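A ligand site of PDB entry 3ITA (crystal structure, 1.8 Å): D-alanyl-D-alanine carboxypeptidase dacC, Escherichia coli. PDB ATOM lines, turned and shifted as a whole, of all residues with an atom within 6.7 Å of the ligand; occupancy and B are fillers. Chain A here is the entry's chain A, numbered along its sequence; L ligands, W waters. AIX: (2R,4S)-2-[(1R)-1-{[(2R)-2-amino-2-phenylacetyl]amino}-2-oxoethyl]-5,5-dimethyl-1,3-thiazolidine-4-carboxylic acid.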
ATOM      1  N   PRO A  38     -23.526  33.467   6.914  1.00  0.00           N
ATOM      2  CA  PRO A  38     -24.796  32.895   6.460  1.00  0.00           C
ATOM      3  C   PRO A  38     -24.961  31.433   6.882  1.00  0.00           C
ATOM      4  O   PRO A  38     -26.088  30.915   6.884  1.00  0.00           O
ATOM      5  CB  PRO A  38     -24.694  32.983   4.930  1.00  0.00           C
ATOM      6  CG  PRO A  38     -23.216  33.001   4.638  1.00  0.00           C
ATOM      7  CD  PRO A  38     -22.630  33.786   5.800  1.00  0.00           C
ATOM      8  N   ALA A  39     -23.856  30.783   7.242  1.00  0.00           N
ATOM      9  CA  ALA A  39     -23.870  29.388   7.699  1.00  0.00           C
ATOM     10  C   ALA A  39     -24.773  28.561   6.773  1.00  0.00           C
ATOM     11  O   ALA A  39     -24.512  28.520   5.573  1.00  0.00           O
ATOM     12  CB  ALA A  39     -24.264  29.288   9.156  1.00  0.00           C
ATOM     13  N   SER A  40     -25.812  27.892   7.274  1.00  0.00           N
ATOM     14  CA  SER A  40     -26.551  26.945   6.381  1.00  0.00           C
ATOM     15  C   SER A  40     -27.203  27.586   5.164  1.00  0.00           C
ATOM     16  O   SER A  40     -27.561  26.899   4.197  1.00  0.00           O
ATOM     17  CB  SER A  40     -27.714  26.291   7.109  1.00  0.00           C
ATOM     18  OG  SER A  40     -27.138  25.355   8.022  1.00  0.00           O
ATOM     19  N   LEU A  41     -27.435  28.886   5.225  1.00  0.00           N
ATOM     20  CA  LEU A  41     -28.092  29.603   4.117  1.00  0.00           C
ATOM     21  C   LEU A  41     -27.196  29.614   2.869  1.00  0.00           C
ATOM     22  O   LEU A  41     -27.637  29.809   1.752  1.00  0.00           O
ATOM     23  CB  LEU A  41     -28.443  31.012   4.569  1.00  0.00           C
ATOM     24  CG  LEU A  41     -29.429  31.140   5.728  1.00  0.00           C
ATOM     25  CD1 LEU A  41     -29.689  32.664   6.050  1.00  0.00           C
ATOM     26  CD2 LEU A  41     -30.761  30.410   5.517  1.00  0.00           C
ATOM     27  N   LYS A  43     -26.230  27.136   1.400  1.00  0.00           N
ATOM     28  CA  LYS A  43     -26.666  26.057   0.528  1.00  0.00           C
ATOM     29  C   LYS A  43     -27.748  26.548  -0.468  1.00  0.00           C
ATOM     30  O   LYS A  43     -28.011  25.885  -1.464  1.00  0.00           O
ATOM     31  CB  LYS A  43     -27.247  24.931   1.391  1.00  0.00           C
ATOM     32  CG  LYS A  43     -26.166  24.128   2.108  1.00  0.00           C
ATOM     33  CD  LYS A  43     -26.757  22.909   2.765  1.00  0.00           C
ATOM     34  CE  LYS A  43     -25.794  22.329   3.794  1.00  0.00           C
ATOM     35  NZ  LYS A  43     -26.146  22.911   5.122  1.00  0.00           N
ATOM     36  N   GLY A  81     -20.610  15.583  12.948  1.00  0.00           N
ATOM     37  CA  GLY A  81     -21.872  15.937  13.606  1.00  0.00           C
ATOM     38  C   GLY A  81     -22.494  17.194  13.028  1.00  0.00           C
ATOM     39  O   GLY A  81     -23.014  18.024  13.751  1.00  0.00           O
ATOM     40  N   SER A  82     -22.414  17.327  11.706  1.00  0.00           N
ATOM     41  CA  SER A  82     -23.318  18.218  10.976  1.00  0.00           C
ATOM     42  C   SER A  82     -24.390  17.398  10.270  1.00  0.00           C
ATOM     43  O   SER A  82     -24.294  16.167  10.215  1.00  0.00           O
ATOM     44  CB  SER A  82     -22.529  19.061   9.971  1.00  0.00           C
ATOM     45  OG  SER A  82     -21.881  18.253   9.004  1.00  0.00           O
ATOM     46  N   SER A  83     -25.413  18.064   9.737  1.00  0.00           N
ATOM     47  CA  SER A  83     -26.403  17.380   8.906  1.00  0.00           C
ATOM     48  C   SER A  83     -25.807  16.673   7.681  1.00  0.00           C
ATOM     49  O   SER A  83     -25.096  17.286   6.879  1.00  0.00           O
ATOM     50  CB  SER A  83     -27.522  18.323   8.489  1.00  0.00           C
ATOM     51  OG  SER A  83     -28.496  17.618   7.735  1.00  0.00           O
ATOM     52  N   SER A 106     -30.631  19.439   3.444  1.00  0.00           N
ATOM     53  CA  SER A 106     -29.467  20.283   3.746  1.00  0.00           C
ATOM     54  C   SER A 106     -28.273  19.472   4.240  1.00  0.00           C
ATOM     55  O   SER A 106     -27.605  19.866   5.202  1.00  0.00           O
ATOM     56  CB  SER A 106     -29.836  21.338   4.802  1.00  0.00           C
ATOM     57  OG  SER A 106     -30.228  22.558   4.196  1.00  0.00           O
ATOM     58  N   ASN A 108     -24.519  18.143   4.395  1.00  0.00           N
ATOM     59  CA  ASN A 108     -23.255  18.786   4.096  1.00  0.00           C
ATOM     60  C   ASN A 108     -22.392  17.878   3.229  1.00  0.00           C
ATOM     61  O   ASN A 108     -21.610  18.361   2.397  1.00  0.00           O
ATOM     62  CB  ASN A 108     -22.542  19.160   5.409  1.00  0.00           C
ATOM     63  CG  ASN A 108     -23.297  20.237   6.200  1.00  0.00           C
ATOM     64  OD1 ASN A 108     -23.911  21.107   5.608  1.00  0.00           O
ATOM     65  ND2 ASN A 108     -23.247  20.163   7.529  1.00  0.00           N
ATOM     66  N   HIS A 147     -20.936  24.136   1.879  1.00  0.00           N
ATOM     67  CA  HIS A 147     -21.986  23.630   2.775  1.00  0.00           C
ATOM     68  C   HIS A 147     -22.432  24.623   3.856  1.00  0.00           C
ATOM     69  O   HIS A 147     -23.359  24.353   4.574  1.00  0.00           O
ATOM     70  CB  HIS A 147     -21.585  22.292   3.441  1.00  0.00           C
ATOM     71  CG  HIS A 147     -20.151  22.232   3.839  1.00  0.00           C
ATOM     72  ND1 HIS A 147     -19.512  23.303   4.438  1.00  0.00           N
ATOM     73  CD2 HIS A 147     -19.201  21.284   3.658  1.00  0.00           C
ATOM     74  CE1 HIS A 147     -18.231  22.994   4.642  1.00  0.00           C
ATOM     75  NE2 HIS A 147     -18.023  21.776   4.160  1.00  0.00           N
ATOM     76  N   GLY A 148     -21.721  25.737   4.004  1.00  0.00           N
ATOM     77  CA  GLY A 148     -22.142  26.772   4.952  1.00  0.00           C
ATOM     78  C   GLY A 148     -21.785  26.443   6.391  1.00  0.00           C
ATOM     79  O   GLY A 148     -22.403  26.943   7.325  1.00  0.00           O
ATOM     80  N   LEU A 149     -20.801  25.563   6.592  1.00  0.00           N
ATOM     81  CA  LEU A 149     -20.256  25.367   7.917  1.00  0.00           C
ATOM     82  C   LEU A 149     -19.618  26.709   8.280  1.00  0.00           C
ATOM     83  O   LEU A 149     -18.887  27.265   7.464  1.00  0.00           O
ATOM     84  CB  LEU A 149     -19.267  24.206   7.910  1.00  0.00           C
ATOM     85  CG  LEU A 149     -19.924  22.821   7.761  1.00  0.00           C
ATOM     86  CD1 LEU A 149     -18.911  21.696   7.573  1.00  0.00           C
ATOM     87  CD2 LEU A 149     -20.899  22.504   8.901  1.00  0.00           C
ATOM     88  N   ASP A 150     -19.963  27.268   9.442  1.00  0.00           N
ATOM     89  CA  ASP A 150     -19.388  28.540   9.869  1.00  0.00           C
ATOM     90  C   ASP A 150     -17.890  28.512   9.542  1.00  0.00           C
ATOM     91  O   ASP A 150     -17.241  27.471   9.686  1.00  0.00           O
ATOM     92  CB  ASP A 150     -19.610  28.806  11.378  1.00  0.00           C
ATOM     93  CG  ASP A 150     -21.094  29.021  11.743  1.00  0.00           C
ATOM     94  OD1 ASP A 150     -21.543  30.190  11.840  1.00  0.00           O
ATOM     95  OD2 ASP A 150     -21.801  28.017  11.960  1.00  0.00           O
ATOM     96  N   ARG A 194     -37.002  20.798   7.005  1.00  0.00           N
ATOM     97  CA  ARG A 194     -37.132  21.563   8.282  1.00  0.00           C
ATOM     98  C   ARG A 194     -37.854  22.902   8.165  1.00  0.00           C
ATOM     99  O   ARG A 194     -38.114  23.551   9.174  1.00  0.00           O
ATOM    100  CB  ARG A 194     -35.770  21.707   8.957  1.00  0.00           C
ATOM    101  CG  ARG A 194     -35.271  20.358   9.503  1.00  0.00           C
ATOM    102  CD  ARG A 194     -34.014  20.537  10.367  1.00  0.00           C
ATOM    103  NE  ARG A 194     -34.318  21.423  11.488  1.00  0.00           N
ATOM    104  CZ  ARG A 194     -34.830  21.004  12.650  1.00  0.00           C
ATOM    105  NH1 ARG A 194     -35.110  21.896  13.601  1.00  0.00           N
ATOM    106  NH2 ARG A 194     -35.065  19.715  12.854  1.00  0.00           N
ATOM    107  N   THR A 210     -33.628  27.097   6.009  1.00  0.00           N
ATOM    108  CA  THR A 210     -33.406  27.487   7.402  1.00  0.00           C
ATOM    109  C   THR A 210     -31.917  27.436   7.756  1.00  0.00           C
ATOM    110  O   THR A 210     -31.127  26.785   7.069  1.00  0.00           O
ATOM    111  CB  THR A 210     -34.142  26.530   8.370  1.00  0.00           C
ATOM    112  OG1 THR A 210     -33.567  25.215   8.261  1.00  0.00           O
ATOM    113  CG2 THR A 210     -35.652  26.483   8.048  1.00  0.00           C
ATOM    114  N   GLY A 211     -31.541  28.119   8.827  1.00  0.00           N
ATOM    115  CA  GLY A 211     -30.168  28.054   9.329  1.00  0.00           C
ATOM    116  C   GLY A 211     -30.027  28.654  10.709  1.00  0.00           C
ATOM    117  O   GLY A 211     -30.952  29.193  11.285  1.00  0.00           O
ATOM    118  N   THR A 212     -28.807  28.599  11.233  1.00  0.00           N
ATOM    119  CA  THR A 212     -28.479  29.351  12.431  1.00  0.00           C
ATOM    120  C   THR A 212     -27.182  30.090  12.144  1.00  0.00           C
ATOM    121  O   THR A 212     -26.423  29.709  11.238  1.00  0.00           O
ATOM    122  CB  THR A 212     -28.226  28.376  13.618  1.00  0.00           C
ATOM    123  OG1 THR A 212     -27.243  27.426  13.223  1.00  0.00           O
ATOM    124  CG2 THR A 212     -29.484  27.627  13.938  1.00  0.00           C
ATOM    125  N   THR A 213     -26.925  31.134  12.933  1.00  0.00           N
ATOM    126  CA  THR A 213     -25.636  31.805  12.926  1.00  0.00           C
ATOM    127  C   THR A 213     -25.092  31.848  14.361  1.00  0.00           C
ATOM    128  O   THR A 213     -25.786  32.278  15.289  1.00  0.00           O
ATOM    129  CB  THR A 213     -25.776  33.243  12.384  1.00  0.00           C
ATOM    130  OG1 THR A 213     -26.168  33.184  10.998  1.00  0.00           O
ATOM    131  CG2 THR A 213     -24.434  33.998  12.485  1.00  0.00           C
ATOM    132  N   TYR A 218     -31.569  32.199  15.169  1.00  0.00           N
ATOM    133  CA  TYR A 218     -32.176  31.303  14.157  1.00  0.00           C
ATOM    134  C   TYR A 218     -32.627  32.096  12.922  1.00  0.00           C
ATOM    135  O   TYR A 218     -33.199  33.185  13.083  1.00  0.00           O
ATOM    136  CB  TYR A 218     -33.394  30.629  14.776  1.00  0.00           C
ATOM    137  CG  TYR A 218     -33.015  29.666  15.914  1.00  0.00           C
ATOM    138  CD1 TYR A 218     -32.879  30.120  17.226  1.00  0.00           C
ATOM    139  CD2 TYR A 218     -32.758  28.317  15.661  1.00  0.00           C
ATOM    140  CE1 TYR A 218     -32.506  29.246  18.262  1.00  0.00           C
ATOM    141  CE2 TYR A 218     -32.388  27.436  16.703  1.00  0.00           C
ATOM    142  CZ  TYR A 218     -32.276  27.902  17.997  1.00  0.00           C
ATOM    143  OH  TYR A 218     -31.919  27.046  19.028  1.00  0.00           O
ATOM    144  N   ASN A 219     -32.352  31.562  11.729  1.00  0.00           N
ATOM    145  CA  ASN A 219     -32.585  32.291  10.457  1.00  0.00           C
ATOM    146  C   ASN A 219     -33.580  31.557   9.546  1.00  0.00           C
ATOM    147  O   ASN A 219     -33.688  30.320   9.590  1.00  0.00           O
ATOM    148  CB  ASN A 219     -31.282  32.410   9.667  1.00  0.00           C
ATOM    149  CG  ASN A 219     -30.138  32.988  10.488  1.00  0.00           C
ATOM    150  OD1 ASN A 219     -30.307  33.837  11.377  1.00  0.00           O
ATOM    151  ND2 ASN A 219     -28.951  32.521  10.191  1.00  0.00           N
ATOM    152  N   ASP A 241     -36.512  28.950  17.555  1.00  0.00           N
ATOM    153  CA  ASP A 241     -37.148  28.317  16.412  1.00  0.00           C
ATOM    154  C   ASP A 241     -38.545  28.857  16.181  1.00  0.00           C
ATOM    155  O   ASP A 241     -38.928  29.157  15.051  1.00  0.00           O
ATOM    156  CB  ASP A 241     -37.166  26.787  16.565  1.00  0.00           C
ATOM    157  CG  ASP A 241     -37.547  26.060  15.249  1.00  0.00           C
ATOM    158  OD1 ASP A 241     -36.863  26.246  14.229  1.00  0.00           O
ATOM    159  OD2 ASP A 241     -38.521  25.292  15.239  1.00  0.00           O
ATOM    160  N   ARG A 244     -38.338  32.484  14.829  1.00  0.00           N
ATOM    161  CA  ARG A 244     -37.819  32.410  13.473  1.00  0.00           C
ATOM    162  C   ARG A 244     -38.963  32.219  12.456  1.00  0.00           C
ATOM    163  O   ARG A 244     -39.004  32.917  11.432  1.00  0.00           O
ATOM    164  CB  ARG A 244     -36.816  31.243  13.409  1.00  0.00           C
ATOM    165  CG  ARG A 244     -36.196  30.947  12.042  1.00  0.00           C
ATOM    166  CD  ARG A 244     -36.497  29.524  11.547  1.00  0.00           C
ATOM    167  NE  ARG A 244     -36.021  28.451  12.434  1.00  0.00           N
ATOM    168  CZ  ARG A 244     -34.796  27.896  12.382  1.00  0.00           C
ATOM    169  NH1 ARG A 244     -33.855  28.332  11.574  1.00  0.00           N
ATOM    170  NH2 ARG A 244     -34.480  26.898  13.208  1.00  0.00           N
HETATM  171  C8  AIX L   1     -27.725  24.175  16.429  1.00  0.00           C
HETATM  172  C5  AIX L   1     -26.034  24.057  14.720  1.00  0.00           C
HETATM  173  C6  AIX L   1     -30.037  22.990  12.285  1.00  0.00           C
HETATM  174  N1  AIX L   1     -26.638  24.937  11.712  1.00  0.00           N
HETATM  175  C2  AIX L   1     -31.342  25.227  12.402  1.00  0.00           C
HETATM  176  N3  AIX L   1     -29.489  24.811  10.790  1.00  0.00           N
HETATM  177  C4  AIX L   1     -25.230  24.734  13.670  1.00  0.00           C
HETATM  178  C1  AIX L   1     -31.249  22.323  11.649  1.00  0.00           C
HETATM  179  C3  AIX L   1     -25.640  24.265  12.294  1.00  0.00           C
HETATM  180  C7  AIX L   1     -26.963  24.787  15.446  1.00  0.00           C
HETATM  181  C9  AIX L   1     -27.543  22.817  16.693  1.00  0.00           C
HETATM  182  C10 AIX L   1     -26.590  22.089  15.988  1.00  0.00           C
HETATM  183  C11 AIX L   1     -25.839  22.705  14.983  1.00  0.00           C
HETATM  184  C12 AIX L   1     -30.041  24.513  12.106  1.00  0.00           C
HETATM  185  C13 AIX L   1     -28.465  23.893  10.316  1.00  0.00           C
HETATM  186  C14 AIX L   1     -27.080  24.552  10.363  1.00  0.00           C
HETATM  187  C15 AIX L   1     -27.074  25.710   9.405  1.00  0.00           C
HETATM  188  C16 AIX L   1     -29.893  22.617  13.757  1.00  0.00           C
HETATM  189  N2  AIX L   1     -23.820  24.450  13.870  1.00  0.00           N
HETATM  190  O1  AIX L   1     -31.900  25.853  11.482  1.00  0.00           O
HETATM  191  O2  AIX L   1     -31.800  25.198  13.569  1.00  0.00           O
HETATM  192  O3  AIX L   1     -25.042  23.321  11.769  1.00  0.00           O
HETATM  193  O4  AIX L   1     -26.986  26.883   9.740  1.00  0.00           O
HETATM  194  S1  AIX L   1     -28.638  22.461  11.364  1.00  0.00           S
HETATM  195  O   HOH W   1     -23.783  25.582   9.266  1.00  0.00           O
HETATM  196  O   HOH W   2     -34.324  24.155  15.302  1.00  0.00           O
HETATM  197  O   HOH W   3     -22.810  25.853  11.588  1.00  0.00           O
HETATM  198  O   HOH W   4     -33.921  24.238  10.703  1.00  0.00           O
HETATM  199  O   HOH W   5     -20.947  24.492  15.481  1.00  0.00           O
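The backbone carbonyl oxygen of Gly 211 lies close to an oxygen (O1) of the ligand, 3.5 Å away.
Ala 39 touches the ligand (CB to O4, 3.7 Å).
Arg 194 touches the ligand (NE to C1, 3.2 Å).
Thr 210 touches the ligand (OG1 to O1, 3.7 Å).
Tyr 218 touches the ligand.
Hydrophobic or aromatic side chains that line the ligand: Ala 39 and Tyr 218.
Within 4 Å of the ligand: Ala 39, Ser 40, Arg 194, Thr 210, Gly 211, Thr 212, Tyr 218 and Arg 244.
NH1 of Arg 244 is in hydrogen-bond range of O of Gly 211.
The guanidinium group of Arg 244 lies within hydrogen-bond range of the backbone carbonyl oxygen of Asn 219, at 2.8 Å.
The guanidinium group of Arg 244 is in salt-bridge range of the side-chain carboxylate of Asp 241, at 2.7 Å.
O of Gly 211 lies within hydrogen-bond range of N of Asn 219, 2.8 Å away.
The backbone NH of Ser 40 sits close to an oxygen (O4) of the ligand, at 2.9 Å.
OG of Ser 40 is bonded to C15 of the ligand, at 1.4 Å.
The backbone NH of Thr 212 is in hydrogen-bond range of an oxygen (O4) of the ligand.
A nitrogen (N1) of the ligand sits at hydrogen-bond distance from the side-chain hydroxyl of Thr 212 (3.0 Å).
NH1 of Arg 244 is in salt-bridge range of O1 of the ligand, 3.2 Å away.
Water W4 lies within hydrogen-bond range of the side-chain hydroxyl of Thr 210 (2.7 Å), an oxygen (O1) of the ligand (2.7 Å) and the guanidinium group of Arg 194 (2.9 Å).
Water W3 lies within hydrogen-bond range of OD2 of Asp 150 and N2 of the ligand.
Water W2 lies within hydrogen-bond range of the guanidinium group (NH1) of Arg 194, an oxygen (O2) of the ligand, the guanidinium group (NH2) of Arg 244 and the side-chain carboxylate (OD1) of Asp 241.
Water W1 lies within hydrogen-bond range of O of Gly 148 and O4 of the ligand.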
